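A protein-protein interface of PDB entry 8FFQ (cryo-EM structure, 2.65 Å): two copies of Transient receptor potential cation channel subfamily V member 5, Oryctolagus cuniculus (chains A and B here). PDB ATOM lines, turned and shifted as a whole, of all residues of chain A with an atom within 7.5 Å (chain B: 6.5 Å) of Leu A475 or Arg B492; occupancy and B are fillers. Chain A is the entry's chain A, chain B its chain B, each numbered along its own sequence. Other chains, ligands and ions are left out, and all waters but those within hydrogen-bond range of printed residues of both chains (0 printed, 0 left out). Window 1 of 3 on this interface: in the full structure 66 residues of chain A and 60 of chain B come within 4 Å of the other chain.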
ATOM      1  N   MET A 466      -8.792   8.320 -16.021  1.00  0.00           N
ATOM      2  CA  MET A 466      -9.684   8.396 -14.858  1.00  0.00           C
ATOM      3  C   MET A 466      -9.803   7.058 -14.077  1.00  0.00           C
ATOM      4  O   MET A 466     -10.209   7.119 -12.917  1.00  0.00           O
ATOM      5  CB  MET A 466     -11.112   8.806 -15.255  1.00  0.00           C
ATOM      6  CG  MET A 466     -11.208  10.141 -16.002  1.00  0.00           C
ATOM      7  SD  MET A 466     -12.921  10.511 -16.473  1.00  0.00           S
ATOM      8  CE  MET A 466     -12.715  11.982 -17.450  1.00  0.00           C
ATOM      9  N   PHE A 468      -7.263   5.703 -12.752  1.00  0.00           N
ATOM     10  CA  PHE A 468      -6.341   6.013 -11.673  1.00  0.00           C
ATOM     11  C   PHE A 468      -6.895   6.998 -10.643  1.00  0.00           C
ATOM     12  O   PHE A 468      -6.339   7.099  -9.555  1.00  0.00           O
ATOM     13  CB  PHE A 468      -4.998   6.448 -12.250  1.00  0.00           C
ATOM     14  CG  PHE A 468      -4.334   5.350 -13.053  1.00  0.00           C
ATOM     15  CD1 PHE A 468      -3.708   4.284 -12.389  1.00  0.00           C
ATOM     16  CD2 PHE A 468      -4.406   5.346 -14.455  1.00  0.00           C
ATOM     17  CE1 PHE A 468      -3.150   3.229 -13.118  1.00  0.00           C
ATOM     18  CE2 PHE A 468      -3.860   4.280 -15.180  1.00  0.00           C
ATOM     19  CZ  PHE A 468      -3.219   3.230 -14.515  1.00  0.00           C
ATOM     20  N   ALA A 469      -8.039   7.638 -10.890  1.00  0.00           N
ATOM     21  CA  ALA A 469      -8.697   8.485  -9.904  1.00  0.00           C
ATOM     22  C   ALA A 469      -9.033   7.726  -8.620  1.00  0.00           C
ATOM     23  O   ALA A 469      -8.956   8.296  -7.540  1.00  0.00           O
ATOM     24  CB  ALA A 469      -9.959   9.073 -10.527  1.00  0.00           C
ATOM     25  N   ARG A 470      -9.218   6.409  -8.720  1.00  0.00           N
ATOM     26  CA  ARG A 470      -9.610   5.529  -7.591  1.00  0.00           C
ATOM     27  C   ARG A 470      -8.534   5.449  -6.526  1.00  0.00           C
ATOM     28  O   ARG A 470      -8.873   5.054  -5.413  1.00  0.00           O
ATOM     29  CB  ARG A 470      -9.874   4.137  -8.141  1.00  0.00           C
ATOM     30  CG  ARG A 470      -8.681   3.289  -8.538  1.00  0.00           C
ATOM     31  CD  ARG A 470      -9.292   2.075  -9.198  1.00  0.00           C
ATOM     32  NE  ARG A 470     -10.183   2.527 -10.250  1.00  0.00           N
ATOM     33  CZ  ARG A 470     -11.358   1.998 -10.559  1.00  0.00           C
ATOM     34  NH1 ARG A 470     -12.078   2.514 -11.537  1.00  0.00           N
ATOM     35  NH2 ARG A 470     -11.819   0.959  -9.894  1.00  0.00           N
ATOM     36  N   GLY A 471      -7.302   5.810  -6.846  1.00  0.00           N
ATOM     37  CA  GLY A 471      -6.186   5.810  -5.909  1.00  0.00           C
ATOM     38  C   GLY A 471      -6.180   6.966  -4.915  1.00  0.00           C
ATOM     39  O   GLY A 471      -5.414   6.933  -3.962  1.00  0.00           O
ATOM     40  N   PHE A 472      -7.007   7.989  -5.115  1.00  0.00           N
ATOM     41  CA  PHE A 472      -6.948   9.251  -4.381  1.00  0.00           C
ATOM     42  C   PHE A 472      -8.325   9.604  -3.843  1.00  0.00           C
ATOM     43  O   PHE A 472      -9.303   9.569  -4.585  1.00  0.00           O
ATOM     44  CB  PHE A 472      -6.424  10.357  -5.310  1.00  0.00           C
ATOM     45  CG  PHE A 472      -5.148  10.009  -6.051  1.00  0.00           C
ATOM     46  CD1 PHE A 472      -3.896  10.229  -5.452  1.00  0.00           C
ATOM     47  CD2 PHE A 472      -5.215   9.450  -7.336  1.00  0.00           C
ATOM     48  CE1 PHE A 472      -2.720   9.894  -6.139  1.00  0.00           C
ATOM     49  CE2 PHE A 472      -4.038   9.116  -8.022  1.00  0.00           C
ATOM     50  CZ  PHE A 472      -2.790   9.343  -7.427  1.00  0.00           C
ATOM     51  N   GLN A 473      -8.420  10.007  -2.580  1.00  0.00           N
ATOM     52  CA  GLN A 473      -9.707  10.335  -1.959  1.00  0.00           C
ATOM     53  C   GLN A 473     -10.363  11.572  -2.585  1.00  0.00           C
ATOM     54  O   GLN A 473     -11.584  11.663  -2.624  1.00  0.00           O
ATOM     55  CB  GLN A 473      -9.513  10.471  -0.448  1.00  0.00           C
ATOM     56  CG  GLN A 473     -10.846  10.536   0.309  1.00  0.00           C
ATOM     57  CD  GLN A 473     -10.686  10.236   1.792  1.00  0.00           C
ATOM     58  OE1 GLN A 473      -9.680  10.533   2.414  1.00  0.00           O
ATOM     59  NE2 GLN A 473     -11.667   9.654   2.432  1.00  0.00           N
ATOM     60  N   MET A 474      -9.578  12.493  -3.153  1.00  0.00           N
ATOM     61  CA  MET A 474     -10.075  13.654  -3.846  1.00  0.00           C
ATOM     62  C   MET A 474     -10.949  13.216  -5.044  1.00  0.00           C
ATOM     63  O   MET A 474     -11.971  13.837  -5.305  1.00  0.00           O
ATOM     64  CB  MET A 474      -8.894  14.558  -4.226  1.00  0.00           C
ATOM     65  CG  MET A 474      -9.435  15.728  -5.041  1.00  0.00           C
ATOM     66  SD  MET A 474      -8.211  17.002  -5.488  1.00  0.00           S
ATOM     67  CE  MET A 474      -8.306  18.080  -4.019  1.00  0.00           C
ATOM     68  N   LEU A 475     -10.520  12.200  -5.802  1.00  0.00           N
ATOM     69  CA  LEU A 475     -11.046  11.953  -7.166  1.00  0.00           C
ATOM     70  C   LEU A 475     -11.831  10.643  -7.313  1.00  0.00           C
ATOM     71  O   LEU A 475     -12.727  10.586  -8.155  1.00  0.00           O
ATOM     72  CB  LEU A 475      -9.865  11.955  -8.162  1.00  0.00           C
ATOM     73  CG  LEU A 475      -8.961  13.168  -8.117  1.00  0.00           C
ATOM     74  CD1 LEU A 475      -7.834  13.022  -9.135  1.00  0.00           C
ATOM     75  CD2 LEU A 475      -9.682  14.423  -8.545  1.00  0.00           C
ATOM     76  N   GLY A 476     -11.557   9.645  -6.486  1.00  0.00           N
ATOM     77  CA  GLY A 476     -12.161   8.324  -6.589  1.00  0.00           C
ATOM     78  C   GLY A 476     -13.674   8.317  -6.407  1.00  0.00           C
ATOM     79  O   GLY A 476     -14.373   7.903  -7.332  1.00  0.00           O
ATOM     80  N   PRO A 477     -14.211   8.832  -5.290  1.00  0.00           N
ATOM     81  CA  PRO A 477     -15.652   8.914  -5.081  1.00  0.00           C
ATOM     82  C   PRO A 477     -16.352   9.709  -6.185  1.00  0.00           C
ATOM     83  O   PRO A 477     -17.375   9.291  -6.713  1.00  0.00           O
ATOM     84  CB  PRO A 477     -15.829   9.532  -3.695  1.00  0.00           C
ATOM     85  CG  PRO A 477     -14.521   9.221  -2.981  1.00  0.00           C
ATOM     86  CD  PRO A 477     -13.499   9.266  -4.104  1.00  0.00           C
ATOM     87  N   PHE A 478     -15.765  10.816  -6.626  1.00  0.00           N
ATOM     88  CA  PHE A 478     -16.314  11.603  -7.715  1.00  0.00           C
ATOM     89  C   PHE A 478     -16.358  10.852  -9.058  1.00  0.00           C
ATOM     90  O   PHE A 478     -17.321  10.973  -9.808  1.00  0.00           O
ATOM     91  CB  PHE A 478     -15.555  12.930  -7.796  1.00  0.00           C
ATOM     92  CG  PHE A 478     -16.134  13.889  -8.807  1.00  0.00           C
ATOM     93  CD1 PHE A 478     -17.525  14.085  -8.879  1.00  0.00           C
ATOM     94  CD2 PHE A 478     -15.296  14.537  -9.725  1.00  0.00           C
ATOM     95  CE1 PHE A 478     -18.075  14.841  -9.921  1.00  0.00           C
ATOM     96  CE2 PHE A 478     -15.851  15.315 -10.755  1.00  0.00           C
ATOM     97  CZ  PHE A 478     -17.242  15.440 -10.870  1.00  0.00           C
ATOM     98  N   THR A 479     -15.390   9.984  -9.336  1.00  0.00           N
ATOM     99  CA  THR A 479     -15.381   9.171 -10.567  1.00  0.00           C
ATOM    100  C   THR A 479     -16.483   8.098 -10.557  1.00  0.00           C
ATOM    101  O   THR A 479     -17.114   7.805 -11.586  1.00  0.00           O
ATOM    102  CB  THR A 479     -14.001   8.570 -10.742  1.00  0.00           C
ATOM    103  OG1 THR A 479     -13.115   9.671 -10.794  1.00  0.00           O
ATOM    104  CG2 THR A 479     -13.797   7.812 -12.051  1.00  0.00           C
ATOM    105  N   ILE A 480     -16.789   7.535  -9.383  1.00  0.00           N
ATOM    106  CA  ILE A 480     -17.965   6.678  -9.185  1.00  0.00           C
ATOM    107  C   ILE A 480     -19.254   7.471  -9.414  1.00  0.00           C
ATOM    108  O   ILE A 480     -20.141   6.995 -10.111  1.00  0.00           O
ATOM    109  CB  ILE A 480     -17.941   6.033  -7.787  1.00  0.00           C
ATOM    110  CG1 ILE A 480     -16.812   4.998  -7.699  1.00  0.00           C
ATOM    111  CG2 ILE A 480     -19.276   5.357  -7.424  1.00  0.00           C
ATOM    112  CD1 ILE A 480     -16.280   4.860  -6.286  1.00  0.00           C
ATOM    113  N   MET A 481     -19.367   8.685  -8.879  1.00  0.00           N
ATOM    114  CA  MET A 481     -20.546   9.515  -9.079  1.00  0.00           C
ATOM    115  C   MET A 481     -20.768   9.827 -10.562  1.00  0.00           C
ATOM    116  O   MET A 481     -21.881   9.648 -11.045  1.00  0.00           O
ATOM    117  CB  MET A 481     -20.460  10.771  -8.208  1.00  0.00           C
ATOM    118  CG  MET A 481     -21.710  11.649  -8.294  1.00  0.00           C
ATOM    119  SD  MET A 481     -23.261  10.935  -7.682  1.00  0.00           S
ATOM    120  CE  MET A 481     -23.052  11.014  -5.895  1.00  0.00           C
ATOM    121  N   ILE A 482     -19.735  10.186 -11.330  1.00  0.00           N
ATOM    122  CA  ILE A 482     -19.861  10.348 -12.785  1.00  0.00           C
ATOM    123  C   ILE A 482     -20.372   9.050 -13.445  1.00  0.00           C
ATOM    124  O   ILE A 482     -21.271   9.050 -14.249  1.00  0.00           O
ATOM    125  CB  ILE A 482     -18.522  10.769 -13.330  1.00  0.00           C
ATOM    126  CG1 ILE A 482     -18.080  12.173 -12.883  1.00  0.00           C
ATOM    127  CG2 ILE A 482     -18.616  10.738 -14.864  1.00  0.00           C
ATOM    128  CD1 ILE A 482     -16.575  12.419 -13.037  1.00  0.00           C
ATOM    129  N   TRP A 593     -16.173   3.524  -3.156  1.00  0.00           N
ATOM    130  CA  TRP A 593     -14.783   3.943  -3.238  1.00  0.00           C
ATOM    131  C   TRP A 593     -13.873   3.156  -2.301  1.00  0.00           C
ATOM    132  O   TRP A 593     -12.829   2.680  -2.736  1.00  0.00           O
ATOM    133  CB  TRP A 593     -14.634   5.441  -3.031  1.00  0.00           C
ATOM    134  CG  TRP A 593     -13.205   5.841  -3.172  1.00  0.00           C
ATOM    135  CD1 TRP A 593     -12.474   5.684  -4.295  1.00  0.00           C
ATOM    136  CD2 TRP A 593     -12.265   6.237  -2.135  1.00  0.00           C
ATOM    137  NE1 TRP A 593     -11.153   5.937  -4.015  1.00  0.00           N
ATOM    138  CE2 TRP A 593     -10.964   6.284  -2.705  1.00  0.00           C
ATOM    139  CE3 TRP A 593     -12.371   6.526  -0.762  1.00  0.00           C
ATOM    140  CZ2 TRP A 593      -9.820   6.585  -1.965  1.00  0.00           C
ATOM    141  CZ3 TRP A 593     -11.229   6.852  -0.010  1.00  0.00           C
ATOM    142  CH2 TRP A 593      -9.959   6.875  -0.604  1.00  0.00           C
ATOM    143  N   GLN A 596     -13.333  -0.073  -4.023  1.00  0.00           N
ATOM    144  CA  GLN A 596     -12.408   0.075  -5.150  1.00  0.00           C
ATOM    145  C   GLN A 596     -10.946   0.123  -4.721  1.00  0.00           C
ATOM    146  O   GLN A 596     -10.097  -0.440  -5.407  1.00  0.00           O
ATOM    147  CB  GLN A 596     -12.694   1.353  -5.942  1.00  0.00           C
ATOM    148  CG  GLN A 596     -13.829   1.212  -6.950  1.00  0.00           C
ATOM    149  CD  GLN A 596     -13.949   2.419  -7.859  1.00  0.00           C
ATOM    150  OE1 GLN A 596     -13.319   3.442  -7.679  1.00  0.00           O
ATOM    151  NE2 GLN A 596     -14.753   2.339  -8.885  1.00  0.00           N
ATOM    152  N   LYS B 484     -13.869  26.972   0.552  1.00  0.00           N
ATOM    153  CA  LYS B 484     -14.120  25.533   0.646  1.00  0.00           C
ATOM    154  C   LYS B 484     -14.517  24.907  -0.698  1.00  0.00           C
ATOM    155  O   LYS B 484     -14.155  23.765  -0.947  1.00  0.00           O
ATOM    156  CB  LYS B 484     -15.123  25.241   1.770  1.00  0.00           C
ATOM    157  CG  LYS B 484     -14.521  25.617   3.134  1.00  0.00           C
ATOM    158  CD  LYS B 484     -15.355  25.189   4.344  1.00  0.00           C
ATOM    159  CE  LYS B 484     -15.419  23.673   4.573  1.00  0.00           C
ATOM    160  NZ  LYS B 484     -14.108  23.079   4.934  1.00  0.00           N
ATOM    161  N   MET B 485     -15.159  25.643  -1.602  1.00  0.00           N
ATOM    162  CA  MET B 485     -15.369  25.204  -2.987  1.00  0.00           C
ATOM    163  C   MET B 485     -14.083  25.184  -3.820  1.00  0.00           C
ATOM    164  O   MET B 485     -13.868  24.211  -4.534  1.00  0.00           O
ATOM    165  CB  MET B 485     -16.452  26.037  -3.682  1.00  0.00           C
ATOM    166  CG  MET B 485     -17.841  25.830  -3.076  1.00  0.00           C
ATOM    167  SD  MET B 485     -18.481  24.141  -3.124  1.00  0.00           S
ATOM    168  CE  MET B 485     -20.115  24.371  -2.402  1.00  0.00           C
ATOM    169  N   ILE B 486     -13.198  26.182  -3.707  1.00  0.00           N
ATOM    170  CA  ILE B 486     -11.912  26.194  -4.427  1.00  0.00           C
ATOM    171  C   ILE B 486     -11.018  25.024  -4.030  1.00  0.00           C
ATOM    172  O   ILE B 486     -10.533  24.304  -4.880  1.00  0.00           O
ATOM    173  CB  ILE B 486     -11.170  27.555  -4.307  1.00  0.00           C
ATOM    174  CG1 ILE B 486     -11.964  28.656  -5.006  1.00  0.00           C
ATOM    175  CG2 ILE B 486      -9.777  27.555  -4.942  1.00  0.00           C
ATOM    176  CD1 ILE B 486     -11.487  30.083  -4.661  1.00  0.00           C
ATOM    177  N   PHE B 487     -10.776  24.839  -2.743  1.00  0.00           N
ATOM    178  CA  PHE B 487      -9.879  23.758  -2.324  1.00  0.00           C
ATOM    179  C   PHE B 487     -10.580  22.389  -2.263  1.00  0.00           C
ATOM    180  O   PHE B 487      -9.974  21.365  -1.941  1.00  0.00           O
ATOM    181  CB  PHE B 487      -9.176  24.132  -1.001  1.00  0.00           C
ATOM    182  CG  PHE B 487      -8.519  25.532  -0.958  1.00  0.00           C
ATOM    183  CD1 PHE B 487      -7.894  26.052  -2.082  1.00  0.00           C
ATOM    184  CD2 PHE B 487      -8.571  26.256   0.241  1.00  0.00           C
ATOM    185  CE1 PHE B 487      -7.297  27.335  -1.991  1.00  0.00           C
ATOM    186  CE2 PHE B 487      -7.957  27.514   0.314  1.00  0.00           C
ATOM    187  CZ  PHE B 487      -7.327  28.061  -0.806  1.00  0.00           C
ATOM    188  N   GLY B 488     -11.878  22.328  -2.506  1.00  0.00           N
ATOM    189  CA  GLY B 488     -12.647  21.095  -2.514  1.00  0.00           C
ATOM    190  C   GLY B 488     -13.117  20.756  -3.900  1.00  0.00           C
ATOM    191  O   GLY B 488     -12.348  20.243  -4.713  1.00  0.00           O
ATOM    192  N   ASP B 489     -14.397  21.016  -4.198  1.00  0.00           N
ATOM    193  CA  ASP B 489     -15.039  20.490  -5.408  1.00  0.00           C
ATOM    194  C   ASP B 489     -14.416  21.065  -6.699  1.00  0.00           C
ATOM    195  O   ASP B 489     -14.400  20.316  -7.671  1.00  0.00           O
ATOM    196  CB  ASP B 489     -16.545  20.781  -5.410  1.00  0.00           C
ATOM    197  CG  ASP B 489     -17.337  19.902  -4.425  1.00  0.00           C
ATOM    198  OD1 ASP B 489     -16.860  18.797  -4.098  1.00  0.00           O
ATOM    199  OD2 ASP B 489     -18.438  20.339  -4.023  1.00  0.00           O
ATOM    200  N   LEU B 490     -13.855  22.288  -6.718  1.00  0.00           N
ATOM    201  CA  LEU B 490     -13.206  22.819  -7.900  1.00  0.00           C
ATOM    202  C   LEU B 490     -11.942  22.054  -8.307  1.00  0.00           C
ATOM    203  O   LEU B 490     -11.866  21.667  -9.469  1.00  0.00           O
ATOM    204  CB  LEU B 490     -12.933  24.312  -7.688  1.00  0.00           C
ATOM    205  CG  LEU B 490     -12.432  25.012  -8.956  1.00  0.00           C
ATOM    206  CD1 LEU B 490     -13.563  25.159  -9.979  1.00  0.00           C
ATOM    207  CD2 LEU B 490     -11.871  26.407  -8.617  1.00  0.00           C
ATOM    208  N   MET B 491     -10.989  21.762  -7.421  1.00  0.00           N
ATOM    209  CA  MET B 491      -9.791  20.960  -7.802  1.00  0.00           C
ATOM    210  C   MET B 491     -10.209  19.573  -8.312  1.00  0.00           C
ATOM    211  O   MET B 491      -9.711  19.063  -9.304  1.00  0.00           O
ATOM    212  CB  MET B 491      -8.905  20.804  -6.586  1.00  0.00           C
ATOM    213  CG  MET B 491      -8.150  22.128  -6.320  1.00  0.00           C
ATOM    214  SD  MET B 491      -6.910  21.920  -5.011  1.00  0.00           S
ATOM    215  CE  MET B 491      -6.416  23.659  -4.894  1.00  0.00           C
ATOM    216  N   ARG B 492     -11.182  18.960  -7.632  1.00  0.00           N
ATOM    217  CA  ARG B 492     -11.617  17.597  -8.049  1.00  0.00           C
ATOM    218  C   ARG B 492     -12.255  17.679  -9.443  1.00  0.00           C
ATOM    219  O   ARG B 492     -11.974  16.781 -10.262  1.00  0.00           O
ATOM    220  CB  ARG B 492     -12.533  16.944  -7.007  1.00  0.00           C
ATOM    221  CG  ARG B 492     -13.893  17.601  -6.841  1.00  0.00           C
ATOM    222  CD  ARG B 492     -14.758  16.776  -5.910  1.00  0.00           C
ATOM    223  NE  ARG B 492     -13.959  16.169  -4.855  1.00  0.00           N
ATOM    224  CZ  ARG B 492     -13.696  16.739  -3.685  1.00  0.00           C
ATOM    225  NH1 ARG B 492     -12.955  16.105  -2.794  1.00  0.00           N
ATOM    226  NH2 ARG B 492     -14.178  17.938  -3.411  1.00  0.00           N
ATOM    227  N   PHE B 493     -13.068  18.709  -9.712  1.00  0.00           N
ATOM    228  CA  PHE B 493     -13.622  18.866 -11.037  1.00  0.00           C
ATOM    229  C   PHE B 493     -12.545  19.192 -12.071  1.00  0.00           C
ATOM    230  O   PHE B 493     -12.548  18.623 -13.153  1.00  0.00           O
ATOM    231  CB  PHE B 493     -14.709  19.927 -10.990  1.00  0.00           C
ATOM    232  CG  PHE B 493     -15.538  19.927 -12.244  1.00  0.00           C
ATOM    233  CD1 PHE B 493     -16.443  18.877 -12.448  1.00  0.00           C
ATOM    234  CD2 PHE B 493     -15.393  20.930 -13.209  1.00  0.00           C
ATOM    235  CE1 PHE B 493     -17.198  18.821 -13.622  1.00  0.00           C
ATOM    236  CE2 PHE B 493     -16.178  20.898 -14.366  1.00  0.00           C
ATOM    237  CZ  PHE B 493     -17.084  19.845 -14.568  1.00  0.00           C
ATOM    238  N   CYS B 494     -11.588  20.058 -11.742  1.00  0.00           N
ATOM    239  CA  CYS B 494     -10.543  20.511 -12.694  1.00  0.00           C
ATOM    240  C   CYS B 494      -9.558  19.429 -13.106  1.00  0.00           C
ATOM    241  O   CYS B 494      -9.132  19.421 -14.273  1.00  0.00           O
ATOM    242  CB  CYS B 494      -9.848  21.776 -12.159  1.00  0.00           C
ATOM    243  SG  CYS B 494     -11.105  23.066 -12.098  1.00  0.00           S
ATOM    244  N   TRP B 495      -9.280  18.440 -12.246  1.00  0.00           N
ATOM    245  CA  TRP B 495      -8.455  17.275 -12.608  1.00  0.00           C
ATOM    246  C   TRP B 495      -9.186  16.400 -13.638  1.00  0.00           C
ATOM    247  O   TRP B 495      -8.579  16.024 -14.662  1.00  0.00           O
ATOM    248  CB  TRP B 495      -8.090  16.432 -11.369  1.00  0.00           C
ATOM    249  CG  TRP B 495      -7.005  16.881 -10.490  1.00  0.00           C
ATOM    250  CD1 TRP B 495      -7.096  17.296  -9.210  1.00  0.00           C
ATOM    251  CD2 TRP B 495      -5.572  17.003 -10.837  1.00  0.00           C
ATOM    252  NE1 TRP B 495      -5.855  17.705  -8.753  1.00  0.00           N
ATOM    253  CE2 TRP B 495      -4.876  17.557  -9.703  1.00  0.00           C
ATOM    254  CE3 TRP B 495      -4.803  16.772 -12.009  1.00  0.00           C
ATOM    255  CZ2 TRP B 495      -3.505  17.811  -9.748  1.00  0.00           C
ATOM    256  CZ3 TRP B 495      -3.454  17.107 -12.062  1.00  0.00           C
ATOM    257  CH2 TRP B 495      -2.780  17.582 -10.922  1.00  0.00           C
ATOM    258  N   LEU B 496     -10.458  16.072 -13.422  1.00  0.00           N
ATOM    259  CA  LEU B 496     -11.187  15.233 -14.363  1.00  0.00           C
ATOM    260  C   LEU B 496     -11.549  15.998 -15.639  1.00  0.00           C
ATOM    261  O   LEU B 496     -11.452  15.446 -16.732  1.00  0.00           O
ATOM    262  CB  LEU B 496     -12.380  14.566 -13.671  1.00  0.00           C
ATOM    263  CG  LEU B 496     -12.011  13.761 -12.407  1.00  0.00           C
ATOM    264  CD1 LEU B 496     -13.168  12.860 -12.022  1.00  0.00           C
ATOM    265  CD2 LEU B 496     -10.799  12.845 -12.559  1.00  0.00           C
ATOM    266  N   MET B 497     -11.840  17.291 -15.532  1.00  0.00           N
ATOM    267  CA  MET B 497     -11.980  18.194 -16.666  1.00  0.00           C
ATOM    268  C   MET B 497     -10.702  18.264 -17.510  1.00  0.00           C
ATOM    269  O   MET B 497     -10.803  18.183 -18.725  1.00  0.00           O
ATOM    270  CB  MET B 497     -12.424  19.571 -16.150  1.00  0.00           C
ATOM    271  CG  MET B 497     -12.516  20.645 -17.231  1.00  0.00           C
ATOM    272  SD  MET B 497     -13.098  22.263 -16.664  1.00  0.00           S
ATOM    273  CE  MET B 497     -11.604  22.941 -15.934  1.00  0.00           C
ATOM    274  N   PHE B 574     -21.155  19.285 -11.850  1.00  0.00           N
ATOM    275  CA  PHE B 574     -20.475  20.237 -10.984  1.00  0.00           C
ATOM    276  C   PHE B 574     -21.442  21.109 -10.152  1.00  0.00           C
ATOM    277  O   PHE B 574     -21.293  21.258  -8.937  1.00  0.00           O
ATOM    278  CB  PHE B 574     -19.526  21.071 -11.842  1.00  0.00           C
ATOM    279  CG  PHE B 574     -18.670  21.976 -11.013  1.00  0.00           C
ATOM    280  CD1 PHE B 574     -17.775  21.431 -10.099  1.00  0.00           C
ATOM    281  CD2 PHE B 574     -18.722  23.372 -11.211  1.00  0.00           C
ATOM    282  CE1 PHE B 574     -16.996  22.270  -9.277  1.00  0.00           C
ATOM    283  CE2 PHE B 574     -17.932  24.197 -10.406  1.00  0.00           C
ATOM    284  CZ  PHE B 574     -17.044  23.662  -9.466  1.00  0.00           C
ATOM    285  N   MET B 577     -22.994  18.594  -7.575  1.00  0.00           N
ATOM    286  CA  MET B 577     -21.976  18.362  -6.563  1.00  0.00           C
ATOM    287  C   MET B 577     -21.831  19.534  -5.592  1.00  0.00           C
ATOM    288  O   MET B 577     -21.947  19.326  -4.391  1.00  0.00           O
ATOM    289  CB  MET B 577     -20.666  18.012  -7.266  1.00  0.00           C
ATOM    290  CG  MET B 577     -19.512  17.870  -6.291  1.00  0.00           C
ATOM    291  SD  MET B 577     -18.065  16.975  -6.876  1.00  0.00           S
ATOM    292  CE  MET B 577     -17.581  17.958  -8.313  1.00  0.00           C
ATOM    293  N   THR B 581     -22.586  19.626  -1.582  1.00  0.00           N
ATOM    294  CA  THR B 581     -21.564  20.121  -0.657  1.00  0.00           C
ATOM    295  C   THR B 581     -22.061  21.304   0.165  1.00  0.00           C
ATOM    296  O   THR B 581     -21.788  21.373   1.358  1.00  0.00           O
ATOM    297  CB  THR B 581     -20.308  20.527  -1.431  1.00  0.00           C
ATOM    298  OG1 THR B 581     -19.707  19.381  -1.959  1.00  0.00           O
ATOM    299  CG2 THR B 581     -19.245  21.235  -0.597  1.00  0.00           C
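Hydrophobic or aromatic side chains of chain A that line the printed part of chain B: Met A466, Met A474, Leu A475, Phe A478 and Ile A482.
Printed residues of chain B that touch a printed residue of chain A: Met B491, Arg B492, Phe B493, Trp B495, Leu B496 and Met B577.
Hydrophobic or aromatic side chains of chain B that line the printed part of chain A: Met B491, Phe B493, Trp B495, Leu B496 and Met B577.
Among the printed residues, 11 pairs touch across the chains.
Among the printed residues, no Asp or Glu carboxylate lies within 4 Å of a Lys or Arg side-chain nitrogen of the other chain.
The backbone carbonyl oxygen (O) of Leu A475 is in hydrogen-bond range of the side-chain hydroxyl (OG1) of Thr A479.
The guanidinium group of Arg B492 lies close to the backbone carbonyl oxygen of Gly B488 (3.2 Å).
The side-chain carboxylate (OD1) of Asp B489 lies within salt-bridge range of the guanidinium group (NH2) of Arg B492.
The side-chain hydroxyl of Thr B581 is in hydrogen-bond range of the backbone carbonyl oxygen of Met B577.
No position is printed for both chains.
The backbone carbonyl oxygen of Met A474 is in hydrogen-bond range of the guanidinium group of Arg B492 (3.1 Å).
Leu B496 touches Met A466 (O to CE, 3.8 Å).
Met A474 touches Met B491.
SD of Met A474 touches CD1 of Trp B495 (3.9 Å).
Arg B492 touches Leu A475.
CD2 of Leu A475 touches CB of Trp B495, 3.8 Å away.
Phe A478 touches Phe B493.
CD2 of Phe A478 touches CD1 of Leu B496, at 3.6 Å.
CE1 of Phe A478 touches CE of Met B577, 3.5 Å away.
Thr A479 touches Leu B496.
Leu B496 touches Ile A482.
Of the printed residues of chain B, Met A466 touches Leu B496 (3.8 Å).
Ala A469 touches none of the printed residues of chain B.
Leu A475 touches two residues of chain B.
Of the printed residues of chain B, Phe A478 touches Phe B493 (3.9 Å), Leu B496 (3.6 Å) and Met B577 (3.5 Å).
Printed residues of chain A within 4 Å of Met B491: Met A474 (3.8 Å).
Arg B492 touches just these residues of chain A: Met A474 (3.1 Å) and Leu A475 (3.7 Å).
The nearest residue of chain B that does not touch Leu A475 is Leu B496 (4.5 Å).
The nearest residue of chain A that does not touch Arg B492 is Phe A478 (4.04 Å).
The nearest printed residue of chain A that does not touch Phe B493 is Leu A475 (5.6 Å).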
